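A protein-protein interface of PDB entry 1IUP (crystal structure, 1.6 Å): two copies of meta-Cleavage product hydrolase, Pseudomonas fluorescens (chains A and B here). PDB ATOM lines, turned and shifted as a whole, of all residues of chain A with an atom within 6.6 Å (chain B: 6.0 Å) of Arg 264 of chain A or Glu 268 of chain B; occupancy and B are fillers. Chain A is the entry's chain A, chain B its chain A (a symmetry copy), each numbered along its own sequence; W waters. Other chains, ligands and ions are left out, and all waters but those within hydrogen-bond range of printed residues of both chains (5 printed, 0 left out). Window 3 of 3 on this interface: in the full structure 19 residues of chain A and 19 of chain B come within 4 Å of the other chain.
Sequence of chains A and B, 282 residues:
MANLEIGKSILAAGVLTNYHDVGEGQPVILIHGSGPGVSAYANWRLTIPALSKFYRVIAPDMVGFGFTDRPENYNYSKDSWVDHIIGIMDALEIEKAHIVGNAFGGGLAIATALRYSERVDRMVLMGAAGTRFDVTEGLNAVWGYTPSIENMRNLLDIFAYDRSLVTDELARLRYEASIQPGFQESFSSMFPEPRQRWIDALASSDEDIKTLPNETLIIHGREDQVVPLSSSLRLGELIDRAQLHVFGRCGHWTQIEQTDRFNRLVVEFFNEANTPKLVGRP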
ATOM      1  N   ALA A  50     -32.789 -16.470   1.971  1.00  0.00           N
ATOM      2  CA  ALA A  50     -32.036 -15.315   2.450  1.00  0.00           C
ATOM      3  C   ALA A  50     -32.908 -14.068   2.587  1.00  0.00           C
ATOM      4  O   ALA A  50     -32.877 -13.387   3.613  1.00  0.00           O
ATOM      5  CB  ALA A  50     -30.861 -15.030   1.511  1.00  0.00           C
ATOM      6  N   LEU A  51     -33.693 -13.777   1.555  1.00  0.00           N
ATOM      7  CA  LEU A  51     -34.553 -12.600   1.570  1.00  0.00           C
ATOM      8  C   LEU A  51     -35.758 -12.704   2.504  1.00  0.00           C
ATOM      9  O   LEU A  51     -36.164 -11.708   3.101  1.00  0.00           O
ATOM     10  CB  LEU A  51     -35.044 -12.285   0.151  1.00  0.00           C
ATOM     11  CG  LEU A  51     -34.118 -11.491  -0.777  1.00  0.00           C
ATOM     12  CD1 LEU A  51     -32.775 -12.194  -0.910  1.00  0.00           C
ATOM     13  CD2 LEU A  51     -34.783 -11.331  -2.143  1.00  0.00           C
ATOM     14  N   THR A 259     -24.213 -16.471  -5.480  1.00  0.00           N
ATOM     15  CA  THR A 259     -25.329 -16.487  -4.540  1.00  0.00           C
ATOM     16  C   THR A 259     -25.212 -15.599  -3.306  1.00  0.00           C
ATOM     17  O   THR A 259     -26.044 -14.716  -3.095  1.00  0.00           O
ATOM     18  CB  THR A 259     -25.615 -17.922  -4.070  1.00  0.00           C
ATOM     19  OG1 THR A 259     -25.809 -18.764  -5.213  1.00  0.00           O
ATOM     20  CG2 THR A 259     -26.871 -17.962  -3.208  1.00  0.00           C
ATOM     21  N   ASP A 260     -24.195 -15.831  -2.483  1.00  0.00           N
ATOM     22  CA  ASP A 260     -24.047 -15.039  -1.270  1.00  0.00           C
ATOM     23  C   ASP A 260     -23.837 -13.555  -1.539  1.00  0.00           C
ATOM     24  O   ASP A 260     -24.411 -12.712  -0.848  1.00  0.00           O
ATOM     25  CB  ASP A 260     -22.915 -15.592  -0.401  1.00  0.00           C
ATOM     26  CG  ASP A 260     -23.214 -16.988   0.121  1.00  0.00           C
ATOM     27  OD1 ASP A 260     -24.409 -17.340   0.238  1.00  0.00           O
ATOM     28  OD2 ASP A 260     -22.257 -17.730   0.426  1.00  0.00           O
ATOM     29  N   ARG A 261     -23.017 -13.230  -2.534  1.00  0.00           N
ATOM     30  CA  ARG A 261     -22.779 -11.830  -2.877  1.00  0.00           C
ATOM     31  C   ARG A 261     -24.068 -11.184  -3.378  1.00  0.00           C
ATOM     32  O   ARG A 261     -24.413 -10.066  -2.985  1.00  0.00           O
ATOM     33  CB  ARG A 261     -21.700 -11.725  -3.954  1.00  0.00           C
ATOM     34  CG  ARG A 261     -20.298 -11.959  -3.429  1.00  0.00           C
ATOM     35  CD  ARG A 261     -19.291 -12.021  -4.560  1.00  0.00           C
ATOM     36  NE  ARG A 261     -17.919 -12.003  -4.058  1.00  0.00           N
ATOM     37  CZ  ARG A 261     -16.842 -12.050  -4.835  1.00  0.00           C
ATOM     38  NH1 ARG A 261     -16.972 -12.124  -6.153  1.00  0.00           N
ATOM     39  NH2 ARG A 261     -15.632 -12.004  -4.294  1.00  0.00           N
ATOM     40  N   PHE A 262     -24.775 -11.902  -4.245  1.00  0.00           N
ATOM     41  CA  PHE A 262     -26.034 -11.426  -4.809  1.00  0.00           C
ATOM     42  C   PHE A 262     -27.063 -11.180  -3.706  1.00  0.00           C
ATOM     43  O   PHE A 262     -27.678 -10.115  -3.642  1.00  0.00           O
ATOM     44  CB  PHE A 262     -26.585 -12.465  -5.793  1.00  0.00           C
ATOM     45  CG  PHE A 262     -27.938 -12.119  -6.350  1.00  0.00           C
ATOM     46  CD1 PHE A 262     -28.063 -11.246  -7.425  1.00  0.00           C
ATOM     47  CD2 PHE A 262     -29.089 -12.668  -5.796  1.00  0.00           C
ATOM     48  CE1 PHE A 262     -29.318 -10.925  -7.943  1.00  0.00           C
ATOM     49  CE2 PHE A 262     -30.352 -12.352  -6.307  1.00  0.00           C
ATOM     50  CZ  PHE A 262     -30.464 -11.481  -7.379  1.00  0.00           C
ATOM     51  N   ASN A 263     -27.247 -12.170  -2.836  1.00  0.00           N
ATOM     52  CA  ASN A 263     -28.213 -12.039  -1.752  1.00  0.00           C
ATOM     53  C   ASN A 263     -27.893 -10.870  -0.829  1.00  0.00           C
ATOM     54  O   ASN A 263     -28.790 -10.126  -0.428  1.00  0.00           O
ATOM     55  CB  ASN A 263     -28.290 -13.336  -0.941  1.00  0.00           C
ATOM     56  CG  ASN A 263     -28.936 -14.472  -1.718  1.00  0.00           C
ATOM     57  OD1 ASN A 263     -29.631 -14.244  -2.710  1.00  0.00           O
ATOM     58  ND2 ASN A 263     -28.726 -15.702  -1.258  1.00  0.00           N
ATOM     59  N   ARG A 264     -26.617 -10.701  -0.501  1.00  0.00           N
ATOM     60  CA  ARG A 264     -26.209  -9.609   0.376  1.00  0.00           C
ATOM     61  C   ARG A 264     -26.479  -8.242  -0.247  1.00  0.00           C
ATOM     62  O   ARG A 264     -26.984  -7.333   0.420  1.00  0.00           O
ATOM     63  CB  ARG A 264     -24.723  -9.734   0.727  1.00  0.00           C
ATOM     64  CG  ARG A 264     -24.443 -10.573   1.963  1.00  0.00           C
ATOM     65  CD  ARG A 264     -22.953 -10.618   2.262  1.00  0.00           C
ATOM     66  NE  ARG A 264     -22.243 -11.549   1.389  1.00  0.00           N
ATOM     67  CZ  ARG A 264     -21.058 -11.303   0.839  1.00  0.00           C
ATOM     68  NH1 ARG A 264     -20.482 -12.210   0.062  1.00  0.00           N
ATOM     69  NH2 ARG A 264     -20.458 -10.140   1.050  1.00  0.00           N
ATOM     70  N   LEU A 265     -26.141  -8.096  -1.523  1.00  0.00           N
ATOM     71  CA  LEU A 265     -26.358  -6.835  -2.224  1.00  0.00           C
ATOM     72  C   LEU A 265     -27.836  -6.482  -2.272  1.00  0.00           C
ATOM     73  O   LEU A 265     -28.220  -5.342  -2.012  1.00  0.00           O
ATOM     74  CB  LEU A 265     -25.823  -6.921  -3.654  1.00  0.00           C
ATOM     75  CG  LEU A 265     -24.318  -6.763  -3.860  1.00  0.00           C
ATOM     76  CD1 LEU A 265     -23.964  -7.108  -5.301  1.00  0.00           C
ATOM     77  CD2 LEU A 265     -23.910  -5.328  -3.533  1.00  0.00           C
ATOM     78  N   VAL A 266     -28.660  -7.467  -2.610  1.00  0.00           N
ATOM     79  CA  VAL A 266     -30.098  -7.256  -2.706  1.00  0.00           C
ATOM     80  C   VAL A 266     -30.723  -6.882  -1.364  1.00  0.00           C
ATOM     81  O   VAL A 266     -31.473  -5.909  -1.280  1.00  0.00           O
ATOM     82  CB  VAL A 266     -30.801  -8.502  -3.284  1.00  0.00           C
ATOM     83  CG1 VAL A 266     -32.306  -8.292  -3.298  1.00  0.00           C
ATOM     84  CG2 VAL A 266     -30.298  -8.765  -4.704  1.00  0.00           C
ATOM     85  N   VAL A 267     -30.408  -7.636  -0.314  1.00  0.00           N
ATOM     86  CA  VAL A 267     -30.953  -7.349   1.012  1.00  0.00           C
ATOM     87  C   VAL A 267     -30.566  -5.954   1.508  1.00  0.00           C
ATOM     88  O   VAL A 267     -31.415  -5.212   2.005  1.00  0.00           O
ATOM     89  CB  VAL A 267     -30.496  -8.404   2.048  1.00  0.00           C
ATOM     90  CG1 VAL A 267     -30.887  -7.963   3.461  1.00  0.00           C
ATOM     91  CG2 VAL A 267     -31.139  -9.746   1.726  1.00  0.00           C
ATOM     92  N   GLU A 268     -29.294  -5.593   1.370  1.00  0.00           N
ATOM     93  CA  GLU A 268     -28.837  -4.275   1.813  1.00  0.00           C
ATOM     94  C   GLU A 268     -29.478  -3.163   0.999  1.00  0.00           C
ATOM     95  O   GLU A 268     -29.778  -2.088   1.524  1.00  0.00           O
ATOM     96  CB  GLU A 268     -27.317  -4.164   1.700  1.00  0.00           C
ATOM     97  CG  GLU A 268     -26.560  -5.117   2.597  1.00  0.00           C
ATOM     98  CD  GLU A 268     -25.066  -4.902   2.518  1.00  0.00           C
ATOM     99  OE1 GLU A 268     -24.527  -4.907   1.390  1.00  0.00           O
ATOM    100  OE2 GLU A 268     -24.430  -4.729   3.582  1.00  0.00           O
ATOM    101  N   PHE A 269     -29.677  -3.426  -0.287  1.00  0.00           N
ATOM    102  CA  PHE A 269     -30.291  -2.459  -1.187  1.00  0.00           C
ATOM    103  C   PHE A 269     -31.727  -2.185  -0.742  1.00  0.00           C
ATOM    104  O   PHE A 269     -32.161  -1.035  -0.694  1.00  0.00           O
ATOM    105  CB  PHE A 269     -30.259  -3.011  -2.618  1.00  0.00           C
ATOM    106  CG  PHE A 269     -30.993  -2.168  -3.627  1.00  0.00           C
ATOM    107  CD1 PHE A 269     -30.607  -0.853  -3.881  1.00  0.00           C
ATOM    108  CD2 PHE A 269     -32.044  -2.709  -4.361  1.00  0.00           C
ATOM    109  CE1 PHE A 269     -31.256  -0.092  -4.859  1.00  0.00           C
ATOM    110  CE2 PHE A 269     -32.701  -1.962  -5.339  1.00  0.00           C
ATOM    111  CZ  PHE A 269     -32.305  -0.649  -5.591  1.00  0.00           C
ATOM    112  N   ARG B 122      -6.525  -8.122  -0.700  1.00  0.00           N
ATOM    113  CA  ARG B 122      -7.609  -7.634  -1.546  1.00  0.00           C
ATOM    114  C   ARG B 122      -7.443  -6.145  -1.824  1.00  0.00           C
ATOM    115  O   ARG B 122      -6.850  -5.421  -1.025  1.00  0.00           O
ATOM    116  CB  ARG B 122      -8.964  -7.898  -0.890  1.00  0.00           C
ATOM    117  CG  ARG B 122      -9.258  -9.380  -0.728  1.00  0.00           C
ATOM    118  CD  ARG B 122     -10.726  -9.650  -0.443  1.00  0.00           C
ATOM    119  NE  ARG B 122     -10.997 -11.087  -0.474  1.00  0.00           N
ATOM    120  CZ  ARG B 122     -12.182 -11.618  -0.757  1.00  0.00           C
ATOM    121  NH1 ARG B 122     -13.216 -10.830  -1.032  1.00  0.00           N
ATOM    122  NH2 ARG B 122     -12.327 -12.936  -0.787  1.00  0.00           N
ATOM    123  N   ASN B 263     -18.975   2.355   2.360  1.00  0.00           N
ATOM    124  CA  ASN B 263     -18.468   1.673   3.545  1.00  0.00           C
ATOM    125  C   ASN B 263     -18.999   0.251   3.667  1.00  0.00           C
ATOM    126  O   ASN B 263     -18.249  -0.670   3.997  1.00  0.00           O
ATOM    127  CB  ASN B 263     -18.810   2.467   4.809  1.00  0.00           C
ATOM    128  CG  ASN B 263     -18.028   3.767   4.911  1.00  0.00           C
ATOM    129  OD1 ASN B 263     -17.000   3.939   4.255  1.00  0.00           O
ATOM    130  ND2 ASN B 263     -18.501   4.680   5.754  1.00  0.00           N
ATOM    131  N   ARG B 264     -20.286   0.069   3.392  1.00  0.00           N
ATOM    132  CA  ARG B 264     -20.889  -1.256   3.478  1.00  0.00           C
ATOM    133  C   ARG B 264     -20.288  -2.227   2.464  1.00  0.00           C
ATOM    134  O   ARG B 264     -19.984  -3.378   2.794  1.00  0.00           O
ATOM    135  CB  ARG B 264     -22.405  -1.167   3.274  1.00  0.00           C
ATOM    136  CG  ARG B 264     -23.193  -0.938   4.554  1.00  0.00           C
ATOM    137  CD  ARG B 264     -24.685  -0.897   4.270  1.00  0.00           C
ATOM    138  NE  ARG B 264     -25.105   0.383   3.705  1.00  0.00           N
ATOM    139  CZ  ARG B 264     -25.978   0.511   2.710  1.00  0.00           C
ATOM    140  NH1 ARG B 264     -26.307   1.715   2.263  1.00  0.00           N
ATOM    141  NH2 ARG B 264     -26.506  -0.567   2.149  1.00  0.00           N
ATOM    142  N   LEU B 265     -20.118  -1.764   1.231  1.00  0.00           N
ATOM    143  CA  LEU B 265     -19.547  -2.600   0.180  1.00  0.00           C
ATOM    144  C   LEU B 265     -18.129  -3.026   0.529  1.00  0.00           C
ATOM    145  O   LEU B 265     -17.768  -4.193   0.380  1.00  0.00           O
ATOM    146  CB  LEU B 265     -19.524  -1.844  -1.149  1.00  0.00           C
ATOM    147  CG  LEU B 265     -20.827  -1.760  -1.941  1.00  0.00           C
ATOM    148  CD1 LEU B 265     -20.656  -0.785  -3.098  1.00  0.00           C
ATOM    149  CD2 LEU B 265     -21.197  -3.150  -2.456  1.00  0.00           C
ATOM    150  N   VAL B 266     -17.330  -2.070   0.990  1.00  0.00           N
ATOM    151  CA  VAL B 266     -15.946  -2.345   1.346  1.00  0.00           C
ATOM    152  C   VAL B 266     -15.826  -3.327   2.510  1.00  0.00           C
ATOM    153  O   VAL B 266     -15.076  -4.300   2.425  1.00  0.00           O
ATOM    154  CB  VAL B 266     -15.193  -1.040   1.682  1.00  0.00           C
ATOM    155  CG1 VAL B 266     -13.776  -1.355   2.131  1.00  0.00           C
ATOM    156  CG2 VAL B 266     -15.160  -0.134   0.450  1.00  0.00           C
ATOM    157  N   VAL B 267     -16.572  -3.088   3.587  1.00  0.00           N
ATOM    158  CA  VAL B 267     -16.529  -3.978   4.746  1.00  0.00           C
ATOM    159  C   VAL B 267     -16.945  -5.408   4.394  1.00  0.00           C
ATOM    160  O   VAL B 267     -16.276  -6.366   4.785  1.00  0.00           O
ATOM    161  CB  VAL B 267     -17.427  -3.453   5.892  1.00  0.00           C
ATOM    162  CG1 VAL B 267     -17.546  -4.504   6.997  1.00  0.00           C
ATOM    163  CG2 VAL B 267     -16.833  -2.170   6.456  1.00  0.00           C
ATOM    164  N   GLU B 268     -18.039  -5.557   3.654  1.00  0.00           N
ATOM    165  CA  GLU B 268     -18.509  -6.888   3.268  1.00  0.00           C
ATOM    166  C   GLU B 268     -17.516  -7.580   2.346  1.00  0.00           C
ATOM    167  O   GLU B 268     -17.336  -8.797   2.411  1.00  0.00           O
ATOM    168  CB  GLU B 268     -19.863  -6.801   2.567  1.00  0.00           C
ATOM    169  CG  GLU B 268     -20.979  -6.279   3.443  1.00  0.00           C
ATOM    170  CD  GLU B 268     -22.314  -6.303   2.734  1.00  0.00           C
ATOM    171  OE1 GLU B 268     -22.399  -5.753   1.616  1.00  0.00           O
ATOM    172  OE2 GLU B 268     -23.278  -6.870   3.295  1.00  0.00           O
ATOM    173  N   PHE B 269     -16.883  -6.794   1.483  1.00  0.00           N
ATOM    174  CA  PHE B 269     -15.897  -7.316   0.545  1.00  0.00           C
ATOM    175  C   PHE B 269     -14.707  -7.885   1.316  1.00  0.00           C
ATOM    176  O   PHE B 269     -14.221  -8.972   1.007  1.00  0.00           O
ATOM    177  CB  PHE B 269     -15.450  -6.189  -0.395  1.00  0.00           C
ATOM    178  CG  PHE B 269     -14.325  -6.562  -1.324  1.00  0.00           C
ATOM    179  CD1 PHE B 269     -14.471  -7.589  -2.254  1.00  0.00           C
ATOM    180  CD2 PHE B 269     -13.130  -5.848  -1.299  1.00  0.00           C
ATOM    181  CE1 PHE B 269     -13.443  -7.895  -3.151  1.00  0.00           C
ATOM    182  CE2 PHE B 269     -12.095  -6.143  -2.187  1.00  0.00           C
ATOM    183  CZ  PHE B 269     -12.252  -7.169  -3.119  1.00  0.00           C
ATOM    184  N   PHE B 270     -14.243  -7.160   2.329  1.00  0.00           N
ATOM    185  CA  PHE B 270     -13.117  -7.645   3.116  1.00  0.00           C
ATOM    186  C   PHE B 270     -13.541  -8.780   4.048  1.00  0.00           C
ATOM    187  O   PHE B 270     -12.749  -9.674   4.342  1.00  0.00           O
ATOM    188  CB  PHE B 270     -12.485  -6.510   3.929  1.00  0.00           C
ATOM    189  CG  PHE B 270     -11.790  -5.466   3.092  1.00  0.00           C
ATOM    190  CD1 PHE B 270     -11.256  -5.783   1.843  1.00  0.00           C
ATOM    191  CD2 PHE B 270     -11.626  -4.171   3.578  1.00  0.00           C
ATOM    192  CE1 PHE B 270     -10.567  -4.825   1.094  1.00  0.00           C
ATOM    193  CE2 PHE B 270     -10.940  -3.210   2.838  1.00  0.00           C
ATOM    194  CZ  PHE B 270     -10.409  -3.539   1.594  1.00  0.00           C
ATOM    195  N   ASN B 271     -14.789  -8.747   4.506  1.00  0.00           N
ATOM    196  CA  ASN B 271     -15.298  -9.788   5.400  1.00  0.00           C
ATOM    197  C   ASN B 271     -15.226 -11.171   4.756  1.00  0.00           C
ATOM    198  O   ASN B 271     -15.103 -12.178   5.453  1.00  0.00           O
ATOM    199  CB  ASN B 271     -16.748  -9.498   5.807  1.00  0.00           C
ATOM    200  CG  ASN B 271     -16.860  -8.441   6.898  1.00  0.00           C
ATOM    201  OD1 ASN B 271     -17.965  -8.039   7.273  1.00  0.00           O
ATOM    202  ND2 ASN B 271     -15.724  -7.992   7.415  1.00  0.00           N
ATOM    203  N   GLU B 272     -15.302 -11.222   3.429  1.00  0.00           N
ATOM    204  CA  GLU B 272     -15.239 -12.494   2.708  1.00  0.00           C
ATOM    205  C   GLU B 272     -13.905 -13.203   2.909  1.00  0.00           C
ATOM    206  O   GLU B 272     -13.848 -14.433   2.936  1.00  0.00           O
ATOM    207  CB  GLU B 272     -15.446 -12.277   1.210  1.00  0.00           C
ATOM    208  CG  GLU B 272     -16.807 -11.756   0.822  1.00  0.00           C
ATOM    209  CD  GLU B 272     -16.918 -11.512  -0.671  1.00  0.00           C
ATOM    210  OE1 GLU B 272     -18.013 -11.124  -1.127  1.00  0.00           O
ATOM    211  OE2 GLU B 272     -15.910 -11.708  -1.390  1.00  0.00           O
ATOM    212  N   ALA B 273     -12.836 -12.422   3.031  1.00  0.00           N
ATOM    213  CA  ALA B 273     -11.494 -12.969   3.217  1.00  0.00           C
ATOM    214  C   ALA B 273     -11.373 -13.745   4.523  1.00  0.00           C
ATOM    215  O   ALA B 273     -10.916 -14.907   4.472  1.00  0.00           O
ATOM    216  CB  ALA B 273     -10.461 -11.845   3.174  1.00  0.00           C
HETATM  217  O   HOH W   1     -28.449  -1.122   3.799  1.00  0.00           O
HETATM  218  O   HOH W   2     -19.706  -8.820  -1.065  1.00  0.00           O
HETATM  219  O   HOH W   3     -26.037  -7.888   3.102  1.00  0.00           O
HETATM  220  O   HOH W   4     -19.316 -10.545   3.359  1.00  0.00           O
HETATM  221  O   HOH W   5     -21.897  -3.981   4.887  1.00  0.00           O
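The side-chain carboxylate (OE2) of Glu 268 of chain B sits close to the side-chain carboxylate (OE2) of Glu 268 of chain A (2.4 Å).
The guanidinium group of Arg 261 of chain A lies within salt-bridge range of the side-chain carboxylate of Glu 272 of chain B, 2.9 Å away.
The guanidinium group (NH1) of Arg 264 of chain A is in salt-bridge range of the side-chain carboxylate (OE1) of Glu 272 of chain B, 2.9 Å away.
OE2 of Glu 272 of chain B lies within salt-bridge range of NH1 of Arg 122 of chain B (2.9 Å).
O of Asp 260 of chain A is in hydrogen-bond range of NE of Arg 264 of chain A.
Among the printed residues, merely in contact across the chains: Leu 265 of chain A with Leu 265 of chain B, Arg 264 of chain A with Glu 268 of chain B and Glu 268 of chain A with Arg 264 of chain B.
Thr 259 of chain A touches none of the printed residues of chain B.
Of the printed residues of chain B, Arg 261 of chain A touches Glu 272.
Of chain B, only Glu 268 (3.7 Å) and Glu 272 (2.9 Å) come within 4 Å of Arg 264 of chain A.
Of the printed residues of chain B, Leu 265 of chain A touches Leu 265 (3.6 Å).
Printed residues of chain A within 4 Å of Arg 264 of chain B: Glu 268.
Of the printed residues of chain A, Leu 265 of chain B touches Leu 265 (3.6 Å).
Of chain A, only Arg 264 (3.7 Å) and Glu 268 (2.3 Å) come within 4 Å of Glu 268 of chain B.
Phe 269 of chain B touches none of the printed residues of chain A.
Printed residues of chain A within 4 Å of Glu 272 of chain B: Arg 261 and Arg 264.
The nearest printed residue of chain B that does not touch Arg 261 of chain A is Arg 122 of chain B (4.2 Å).
Of the 12 printed residues of chain B, 4 touch a printed residue of chain A.
Hydrophobic or aromatic side chains of chain B that line the printed part of chain A: Leu 265.
Of the 13 printed residues of chain A, 4 touch a printed residue of chain B.
Printed residues of chain A that touch a printed residue of chain B: Arg 261, Arg 264, Leu 265 and Glu 268.
Hydrophobic or aromatic side chains of chain A that line the printed part of chain B: Leu 265.
Among the printed residues, 6 pairs touch across the chains.
Arg 264 of chain A touches Glu 268 of chain B, and with the chains exchanged Glu 268 of chain A touches Arg 264 of chain B.
Leu 265 of chain B touches its own counterpart, Leu 265 of chain A.
Glu 268 of chain B touches its own counterpart, Glu 268 of chain A.
Positions printed for both chains: 263, 264, 265, 266, 267, 268 and 269.
Of the 6 pairs that touch across the chains among the printed residues, 4 have their exchanged pair printed and touching as well.
Water W2 lies within hydrogen-bond range of NH2 of Arg 264 of chain A and OE1 of Glu 272 of chain B.
Water W1 lies within hydrogen-bond range of NH2 of Arg 264 of chain B (2.6 Å) and O of Glu 268 of chain A (2.8 Å).
Water W4 bridges the guanidinium group (NH2) of Arg 264 of chain A (2.6 Å) and the backbone carbonyl oxygen (O) of Glu 268 of chain B (2.8 Å).
Water W3 lies within hydrogen-bond range of O of Arg 264 of chain A (2.9 Å) and OE2 of Glu 268 of chain B (2.9 Å).
Water W5 bridges the backbone carbonyl oxygen of Arg 264 of chain B (2.9 Å) and the side-chain carboxylate of Glu 268 of chain A (2.9 Å).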
